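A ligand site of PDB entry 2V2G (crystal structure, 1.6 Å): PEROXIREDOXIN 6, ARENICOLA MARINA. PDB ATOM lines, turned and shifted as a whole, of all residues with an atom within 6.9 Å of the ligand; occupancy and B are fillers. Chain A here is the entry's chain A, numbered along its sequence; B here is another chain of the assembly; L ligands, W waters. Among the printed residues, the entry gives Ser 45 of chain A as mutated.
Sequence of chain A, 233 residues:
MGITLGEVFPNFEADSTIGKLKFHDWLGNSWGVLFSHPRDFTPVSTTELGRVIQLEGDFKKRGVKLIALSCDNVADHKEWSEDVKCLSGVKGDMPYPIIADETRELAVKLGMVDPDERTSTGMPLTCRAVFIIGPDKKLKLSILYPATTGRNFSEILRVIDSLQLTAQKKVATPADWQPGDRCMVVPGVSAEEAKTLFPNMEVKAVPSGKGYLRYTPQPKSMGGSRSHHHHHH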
ATOM      1  N   HIS A  37      15.478  23.575 -21.106  1.00  0.00           N
ATOM      2  CA  HIS A  37      15.316  24.095 -19.783  1.00  0.00           C
ATOM      3  C   HIS A  37      14.412  23.203 -18.937  1.00  0.00           C
ATOM      4  O   HIS A  37      13.637  22.407 -19.470  1.00  0.00           O
ATOM      5  CB  HIS A  37      14.753  25.524 -19.803  1.00  0.00           C
ATOM      6  CG  HIS A  37      13.340  25.589 -20.312  1.00  0.00           C
ATOM      7  ND1 HIS A  37      13.036  25.599 -21.654  1.00  0.00           N
ATOM      8  CD2 HIS A  37      12.154  25.662 -19.651  1.00  0.00           C
ATOM      9  CE1 HIS A  37      11.715  25.620 -21.801  1.00  0.00           C
ATOM     10  NE2 HIS A  37      11.151  25.619 -20.607  1.00  0.00           N
ATOM     11  N   PRO A  38      14.556  23.260 -17.595  1.00  0.00           N
ATOM     12  CA  PRO A  38      13.858  22.266 -16.746  1.00  0.00           C
ATOM     13  C   PRO A  38      12.335  22.324 -16.731  1.00  0.00           C
ATOM     14  O   PRO A  38      11.688  21.297 -16.892  1.00  0.00           O
ATOM     15  CB  PRO A  38      14.478  22.482 -15.360  1.00  0.00           C
ATOM     16  CG  PRO A  38      15.754  23.188 -15.621  1.00  0.00           C
ATOM     17  CD  PRO A  38      15.543  24.047 -16.815  1.00  0.00           C
ATOM     18  N   ARG A  39      11.763  23.522 -16.627  1.00  0.00           N
ATOM     19  CA  ARG A  39      10.347  23.653 -16.420  1.00  0.00           C
ATOM     20  C   ARG A  39       9.904  25.047 -16.869  1.00  0.00           C
ATOM     21  O   ARG A  39      10.564  26.009 -16.597  1.00  0.00           O
ATOM     22  CB  ARG A  39       9.998  23.463 -14.912  1.00  0.00           C
ATOM     23  CG  ARG A  39       8.597  23.054 -14.674  1.00  0.00           C
ATOM     24  CD  ARG A  39       8.536  21.609 -14.905  1.00  0.00           C
ATOM     25  NE  ARG A  39       7.196  21.058 -14.888  1.00  0.00           N
ATOM     26  CZ  ARG A  39       6.583  20.654 -13.770  1.00  0.00           C
ATOM     27  NH1 ARG A  39       7.163  20.782 -12.572  1.00  0.00           N
ATOM     28  NH2 ARG A  39       5.357  20.145 -13.862  1.00  0.00           N
ATOM     29  N   PHE A  41       7.442  28.341 -16.530  1.00  0.00           N
ATOM     30  CA  PHE A  41       6.995  29.070 -15.359  1.00  0.00           C
ATOM     31  C   PHE A  41       7.994  28.939 -14.179  1.00  0.00           C
ATOM     32  O   PHE A  41       7.579  28.796 -13.001  1.00  0.00           O
ATOM     33  CB  PHE A  41       5.564  28.677 -14.878  1.00  0.00           C
ATOM     34  CG  PHE A  41       4.456  28.723 -15.946  1.00  0.00           C
ATOM     35  CD1 PHE A  41       3.972  29.932 -16.445  1.00  0.00           C
ATOM     36  CD2 PHE A  41       3.907  27.554 -16.433  1.00  0.00           C
ATOM     37  CE1 PHE A  41       2.978  29.976 -17.406  1.00  0.00           C
ATOM     38  CE2 PHE A  41       2.900  27.583 -17.388  1.00  0.00           C
ATOM     39  CZ  PHE A  41       2.421  28.805 -17.876  1.00  0.00           C
ATOM     40  N   THR A  42       9.271  28.948 -14.507  1.00  0.00           N
ATOM     41  CA  THR A  42      10.312  29.055 -13.505  1.00  0.00           C
ATOM     42  C   THR A  42      11.248  30.195 -13.876  1.00  0.00           C
ATOM     43  O   THR A  42      11.374  30.544 -15.075  1.00  0.00           O
ATOM     44  CB  THR A  42      11.034  27.732 -13.341  1.00  0.00           C
ATOM     45  OG1 THR A  42      11.677  27.419 -14.592  1.00  0.00           O
ATOM     46  CG2 THR A  42      10.072  26.654 -12.898  1.00  0.00           C
ATOM     47  N   PRO A  43      11.863  30.830 -12.837  1.00  0.00           N
ATOM     48  CA  PRO A  43      12.480  32.168 -13.013  1.00  0.00           C
ATOM     49  C   PRO A  43      13.732  32.209 -13.884  1.00  0.00           C
ATOM     50  O   PRO A  43      13.829  33.014 -14.812  1.00  0.00           O
ATOM     51  CB  PRO A  43      12.730  32.658 -11.565  1.00  0.00           C
ATOM     52  CG  PRO A  43      12.753  31.404 -10.751  1.00  0.00           C
ATOM     53  CD  PRO A  43      11.793  30.434 -11.409  1.00  0.00           C
ATOM     54  N   VAL A  44      14.743  31.403 -13.560  1.00  0.00           N
ATOM     55  CA  VAL A  44      15.976  31.409 -14.425  1.00  0.00           C
ATOM     56  C   VAL A  44      15.655  31.098 -15.875  1.00  0.00           C
ATOM     57  O   VAL A  44      16.163  31.736 -16.767  1.00  0.00           O
ATOM     58  CB  VAL A  44      17.104  30.483 -13.859  1.00  0.00           C
ATOM     59  CG1 VAL A  44      18.259  30.263 -14.898  1.00  0.00           C
ATOM     60  CG2 VAL A  44      17.611  31.095 -12.490  1.00  0.00           C
ATOM     61  N   SER A  45      14.807  30.083 -16.054  1.00  0.00           N
ATOM     62  CA  SER A  45      14.387  29.651 -17.392  1.00  0.00           C
ATOM     63  C   SER A  45      13.767  30.826 -18.155  1.00  0.00           C
ATOM     64  O   SER A  45      14.023  30.997 -19.363  1.00  0.00           O
ATOM     65  CB  SER A  45      13.402  28.520 -17.343  1.00  0.00           C
ATOM     66  OG  SER A  45      14.006  27.342 -16.817  1.00  0.00           O
ATOM     67  N   THR A  46      13.010  31.628 -17.434  1.00  0.00           N
ATOM     68  CA  THR A  46      12.361  32.812 -18.049  1.00  0.00           C
ATOM     69  C   THR A  46      13.418  33.821 -18.465  1.00  0.00           C
ATOM     70  O   THR A  46      13.404  34.349 -19.601  1.00  0.00           O
ATOM     71  CB  THR A  46      11.284  33.443 -17.150  1.00  0.00           C
ATOM     72  OG1 THR A  46      10.370  32.458 -16.711  1.00  0.00           O
ATOM     73  CG2 THR A  46      10.400  34.534 -17.896  1.00  0.00           C
ATOM     74  N   GLU A  48      16.475  33.164 -19.283  1.00  0.00           N
ATOM     75  CA  GLU A  48      17.239  32.586 -20.386  1.00  0.00           C
ATOM     76  C   GLU A  48      16.525  32.665 -21.732  1.00  0.00           C
ATOM     77  O   GLU A  48      17.113  33.202 -22.723  1.00  0.00           O
ATOM     78  CB  GLU A  48      17.565  31.142 -20.086  1.00  0.00           C
ATOM     79  CG  GLU A  48      18.619  31.005 -19.021  1.00  0.00           C
ATOM     80  CD  GLU A  48      18.973  29.529 -18.859  1.00  0.00           C
ATOM     81  OE1 GLU A  48      18.027  28.745 -18.841  1.00  0.00           O
ATOM     82  OE2 GLU A  48      20.177  29.188 -18.865  1.00  0.00           O
ATOM     83  N   ASP A 114      18.213  16.359 -15.683  1.00  0.00           N
ATOM     84  CA  ASP A 114      18.785  17.140 -14.561  1.00  0.00           C
ATOM     85  C   ASP A 114      18.971  16.204 -13.376  1.00  0.00           C
ATOM     86  O   ASP A 114      18.121  15.369 -13.047  1.00  0.00           O
ATOM     87  CB  ASP A 114      17.871  18.304 -14.176  1.00  0.00           C
ATOM     88  CG  ASP A 114      18.572  19.333 -13.308  1.00  0.00           C
ATOM     89  OD1 ASP A 114      19.197  20.225 -13.928  1.00  0.00           O
ATOM     90  OD2 ASP A 114      18.486  19.174 -12.047  1.00  0.00           O
ATOM     91  N   GLU A 117      16.394  18.197 -10.269  1.00  0.00           N
ATOM     92  CA  GLU A 117      15.042  18.758 -10.448  1.00  0.00           C
ATOM     93  C   GLU A 117      14.176  17.683 -11.071  1.00  0.00           C
ATOM     94  O   GLU A 117      14.439  17.234 -12.186  1.00  0.00           O
ATOM     95  CB  GLU A 117      15.018  20.006 -11.321  1.00  0.00           C
ATOM     96  CG  GLU A 117      15.654  21.196 -10.684  1.00  0.00           C
ATOM     97  CD  GLU A 117      15.061  21.522  -9.320  1.00  0.00           C
ATOM     98  OE1 GLU A 117      13.798  21.553  -9.230  1.00  0.00           O
ATOM     99  OE2 GLU A 117      15.841  21.757  -8.343  1.00  0.00           O
ATOM    100  N   LEU A 125      13.219  15.667 -15.427  1.00  0.00           N
ATOM    101  CA  LEU A 125      13.137  16.899 -16.175  1.00  0.00           C
ATOM    102  C   LEU A 125      14.502  17.134 -16.804  1.00  0.00           C
ATOM    103  O   LEU A 125      15.515  16.550 -16.379  1.00  0.00           O
ATOM    104  CB  LEU A 125      12.814  18.077 -15.272  1.00  0.00           C
ATOM    105  CG  LEU A 125      11.421  18.121 -14.644  1.00  0.00           C
ATOM    106  CD1 LEU A 125      11.447  19.176 -13.498  1.00  0.00           C
ATOM    107  CD2 LEU A 125      10.347  18.397 -15.782  1.00  0.00           C
ATOM    108  N   ARG A 128      19.843  22.324 -18.342  1.00  0.00           N
ATOM    109  CA  ARG A 128      20.006  23.447 -19.205  1.00  0.00           C
ATOM    110  C   ARG A 128      21.065  23.093 -20.241  1.00  0.00           C
ATOM    111  O   ARG A 128      22.266  23.410 -20.103  1.00  0.00           O
ATOM    112  CB  ARG A 128      20.396  24.651 -18.384  1.00  0.00           C
ATOM    113  CG  ARG A 128      19.353  25.152 -17.429  1.00  0.00           C
ATOM    114  CD  ARG A 128      19.707  26.428 -16.717  1.00  0.00           C
ATOM    115  NE  ARG A 128      18.816  26.596 -15.585  1.00  0.00           N
ATOM    116  CZ  ARG A 128      17.517  26.895 -15.622  1.00  0.00           C
ATOM    117  NH1 ARG A 128      16.942  27.229 -16.757  1.00  0.00           N
ATOM    118  NH2 ARG A 128      16.802  26.795 -14.529  1.00  0.00           N
ATOM    119  N   ALA A 147      20.132  22.810 -13.444  1.00  0.00           N
ATOM    120  CA  ALA A 147      19.048  23.738 -13.249  1.00  0.00           C
ATOM    121  C   ALA A 147      19.447  24.980 -12.451  1.00  0.00           C
ATOM    122  O   ALA A 147      18.892  26.035 -12.601  1.00  0.00           O
ATOM    123  CB  ALA A 147      17.884  23.016 -12.575  1.00  0.00           C
ATOM    124  N   THR A 148      20.409  24.837 -11.544  1.00  0.00           N
ATOM    125  CA  THR A 148      20.839  25.918 -10.671  1.00  0.00           C
ATOM    126  C   THR A 148      21.496  27.115 -11.383  1.00  0.00           C
ATOM    127  O   THR A 148      21.643  28.205 -10.809  1.00  0.00           O
ATOM    128  CB  THR A 148      21.977  25.404  -9.676  1.00  0.00           C
ATOM    129  OG1 THR A 148      23.115  24.845 -10.378  1.00  0.00           O
ATOM    130  CG2 THR A 148      21.418  24.402  -8.676  1.00  0.00           C
ATOM    131  N   VAL B 171      18.771  29.586  -4.010  1.00  0.00           N
ATOM    132  CA  VAL B 171      18.746  30.468  -5.123  1.00  0.00           C
ATOM    133  C   VAL B 171      19.269  29.742  -6.374  1.00  0.00           C
ATOM    134  O   VAL B 171      19.879  28.641  -6.264  1.00  0.00           O
ATOM    135  CB  VAL B 171      19.559  31.743  -4.861  1.00  0.00           C
ATOM    136  CG1 VAL B 171      19.032  32.479  -3.630  1.00  0.00           C
ATOM    137  CG2 VAL B 171      21.052  31.402  -4.793  1.00  0.00           C
ATOM    138  N   ALA B 172      19.003  30.353  -7.524  1.00  0.00           N
ATOM    139  CA  ALA B 172      19.565  29.931  -8.813  1.00  0.00           C
ATOM    140  C   ALA B 172      19.971  31.187  -9.567  1.00  0.00           C
ATOM    141  O   ALA B 172      19.360  32.262  -9.445  1.00  0.00           O
ATOM    142  CB  ALA B 172      18.533  29.118  -9.617  1.00  0.00           C
ATOM    143  N   THR B 173      21.044  31.074 -10.342  1.00  0.00           N
ATOM    144  CA  THR B 173      21.635  32.232 -10.974  1.00  0.00           C
ATOM    145  C   THR B 173      21.046  32.449 -12.398  1.00  0.00           C
ATOM    146  O   THR B 173      20.925  31.481 -13.181  1.00  0.00           O
ATOM    147  CB  THR B 173      23.188  32.160 -10.996  1.00  0.00           C
ATOM    148  OG1 THR B 173      23.620  30.993 -11.728  1.00  0.00           O
ATOM    149  CG2 THR B 173      23.743  32.090  -9.542  1.00  0.00           C
ATOM    150  N   MET B 184      17.858  34.487  -8.425  1.00  0.00           N
ATOM    151  CA  MET B 184      16.469  34.128  -8.399  1.00  0.00           C
ATOM    152  C   MET B 184      16.189  33.188  -7.252  1.00  0.00           C
ATOM    153  O   MET B 184      16.936  32.253  -7.000  1.00  0.00           O
ATOM    154  CB  MET B 184      16.082  33.377  -9.649  1.00  0.00           C
ATOM    155  CG  MET B 184      16.428  34.049 -10.980  1.00  0.00           C
ATOM    156  SD  MET B 184      16.097  35.788 -11.142  1.00  0.00           S
ATOM    157  CE  MET B 184      14.383  35.747 -11.015  1.00  0.00           C
ATOM    158  N   VAL B 185      15.080  33.421  -6.567  1.00  0.00           N
ATOM    159  CA  VAL B 185      14.652  32.531  -5.513  1.00  0.00           C
ATOM    160  C   VAL B 185      14.061  31.257  -6.166  1.00  0.00           C
ATOM    161  O   VAL B 185      13.221  31.345  -7.095  1.00  0.00           O
ATOM    162  CB  VAL B 185      13.632  33.221  -4.581  1.00  0.00           C
ATOM    163  CG1 VAL B 185      13.138  32.239  -3.523  1.00  0.00           C
ATOM    164  CG2 VAL B 185      14.274  34.466  -3.928  1.00  0.00           C
ATOM    165  N   VAL B 186      14.510  30.084  -5.723  1.00  0.00           N
ATOM    166  CA  VAL B 186      14.053  28.859  -6.378  1.00  0.00           C
ATOM    167  C   VAL B 186      12.548  28.664  -6.082  1.00  0.00           C
ATOM    168  O   VAL B 186      12.069  29.068  -5.033  1.00  0.00           O
ATOM    169  CB  VAL B 186      14.866  27.593  -5.955  1.00  0.00           C
ATOM    170  CG1 VAL B 186      16.370  27.725  -6.318  1.00  0.00           C
ATOM    171  CG2 VAL B 186      14.661  27.318  -4.464  1.00  0.00           C
ATOM    172  N   PRO B 187      11.826  28.003  -7.026  1.00  0.00           N
ATOM    173  CA  PRO B 187      10.383  27.854  -6.913  1.00  0.00           C
ATOM    174  C   PRO B 187       9.958  27.167  -5.619  1.00  0.00           C
ATOM    175  O   PRO B 187       8.920  27.496  -5.069  1.00  0.00           O
ATOM    176  CB  PRO B 187      10.028  26.951  -8.099  1.00  0.00           C
ATOM    177  CG  PRO B 187      11.102  27.153  -9.087  1.00  0.00           C
ATOM    178  CD  PRO B 187      12.328  27.377  -8.273  1.00  0.00           C
ATOM    179  N   GLY B 188      10.736  26.177  -5.182  1.00  0.00           N
ATOM    180  CA  GLY B 188      10.437  25.427  -3.962  1.00  0.00           C
ATOM    181  C   GLY B 188      10.208  26.217  -2.678  1.00  0.00           C
ATOM    182  O   GLY B 188       9.568  25.712  -1.758  1.00  0.00           O
ATOM    183  N   TYR B 212       6.173  33.299  -9.561  1.00  0.00           N
ATOM    184  CA  TYR B 212       7.487  32.640  -9.597  1.00  0.00           C
ATOM    185  C   TYR B 212       8.694  33.532  -9.955  1.00  0.00           C
ATOM    186  O   TYR B 212       9.827  33.111  -9.741  1.00  0.00           O
ATOM    187  CB  TYR B 212       7.453  31.457 -10.593  1.00  0.00           C
ATOM    188  CG  TYR B 212       7.287  31.912 -12.024  1.00  0.00           C
ATOM    189  CD1 TYR B 212       8.402  32.231 -12.773  1.00  0.00           C
ATOM    190  CD2 TYR B 212       6.050  31.974 -12.626  1.00  0.00           C
ATOM    191  CE1 TYR B 212       8.288  32.653 -14.065  1.00  0.00           C
ATOM    192  CE2 TYR B 212       5.906  32.395 -13.911  1.00  0.00           C
ATOM    193  CZ  TYR B 212       7.066  32.711 -14.641  1.00  0.00           C
ATOM    194  OH  TYR B 212       6.970  33.127 -15.944  1.00  0.00           O
HETATM  195  C1  LIG L   1      14.572  28.132 -12.545  1.00  0.00           C
HETATM  196  O1  LIG L   1      14.696  29.085 -11.648  1.00  0.00           O
HETATM  197  O2  LIG L   1      14.422  28.219 -13.840  1.00  0.00           O
HETATM  198  C2  LIG L   1      14.588  26.805 -11.878  1.00  0.00           C
HETATM  199  C3  LIG L   1      13.998  25.719 -12.492  1.00  0.00           C
HETATM  200  C4  LIG L   1      14.002  24.511 -11.859  1.00  0.00           C
HETATM  201  C5  LIG L   1      14.541  24.406 -10.577  1.00  0.00           C
HETATM  202  C6  LIG L   1      15.159  25.490  -9.944  1.00  0.00           C
HETATM  203  C7  LIG L   1      15.174  26.715 -10.598  1.00  0.00           C
HETATM  204  O   HOH W   1      13.133  25.547 -15.216  1.00  0.00           O
HETATM  205  O   HOH W   2      17.924  24.976  -8.360  1.00  0.00           O
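Water W1 lies within hydrogen-bond range of OG1 of Thr 42 (2.5 Å), OG of Ser 45 (2.6 Å), N of Arg 39 (2.8 Å) and O2 of the ligand (3.3 Å).
Pro 43 touches the ligand (CG to O1, 3.2 Å).
Glu 117 touches the ligand.
Pro 187 of chain B touches the ligand.
Hydrophobic or aromatic side chains that line the ligand: Pro 43, Val 44 and Pro 187 of chain B.
The nearest printed residue that does not touch the ligand is Pro 38 (4.1 Å).
NH1 of Arg 128 sits at hydrogen-bond distance from OG of Ser 45 (2.9 Å).
NH2 of Arg 128 is in hydrogen-bond range of O of Ala 147 (2.9 Å).
The guanidinium group of Arg 128 is in salt-bridge range of the side-chain carboxylate of Glu 48 (2.8 Å).
OG of Ser 45 sits at hydrogen-bond distance from OG1 of Thr 42 (3.2 Å).
The side-chain hydroxyl of Thr 42 lies within hydrogen-bond range of the backbone carbonyl oxygen of Arg 39, 2.7 Å away.
OG1 of Thr 46 is in hydrogen-bond range of O of Thr 42 (2.7 Å).
The backbone NH of Glu 117 is in hydrogen-bond range of the side-chain carboxylate of Asp 114, 2.9 Å away.
NH2 of Arg 128 is in salt-bridge range of O2 of the ligand.
O2 of the ligand sits at hydrogen-bond distance from N of Ser 45 (2.9 Å).
OG of Ser 45 sits at hydrogen-bond distance from O2 of the ligand (3.1 Å).
The side-chain hydroxyl (OG1) of Thr 42 is in hydrogen-bond range of an oxygen (O2) of the ligand (3.0 Å).
The backbone NH (N) of Val 44 sits at hydrogen-bond distance from an oxygen (O1) of the ligand (3.0 Å).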
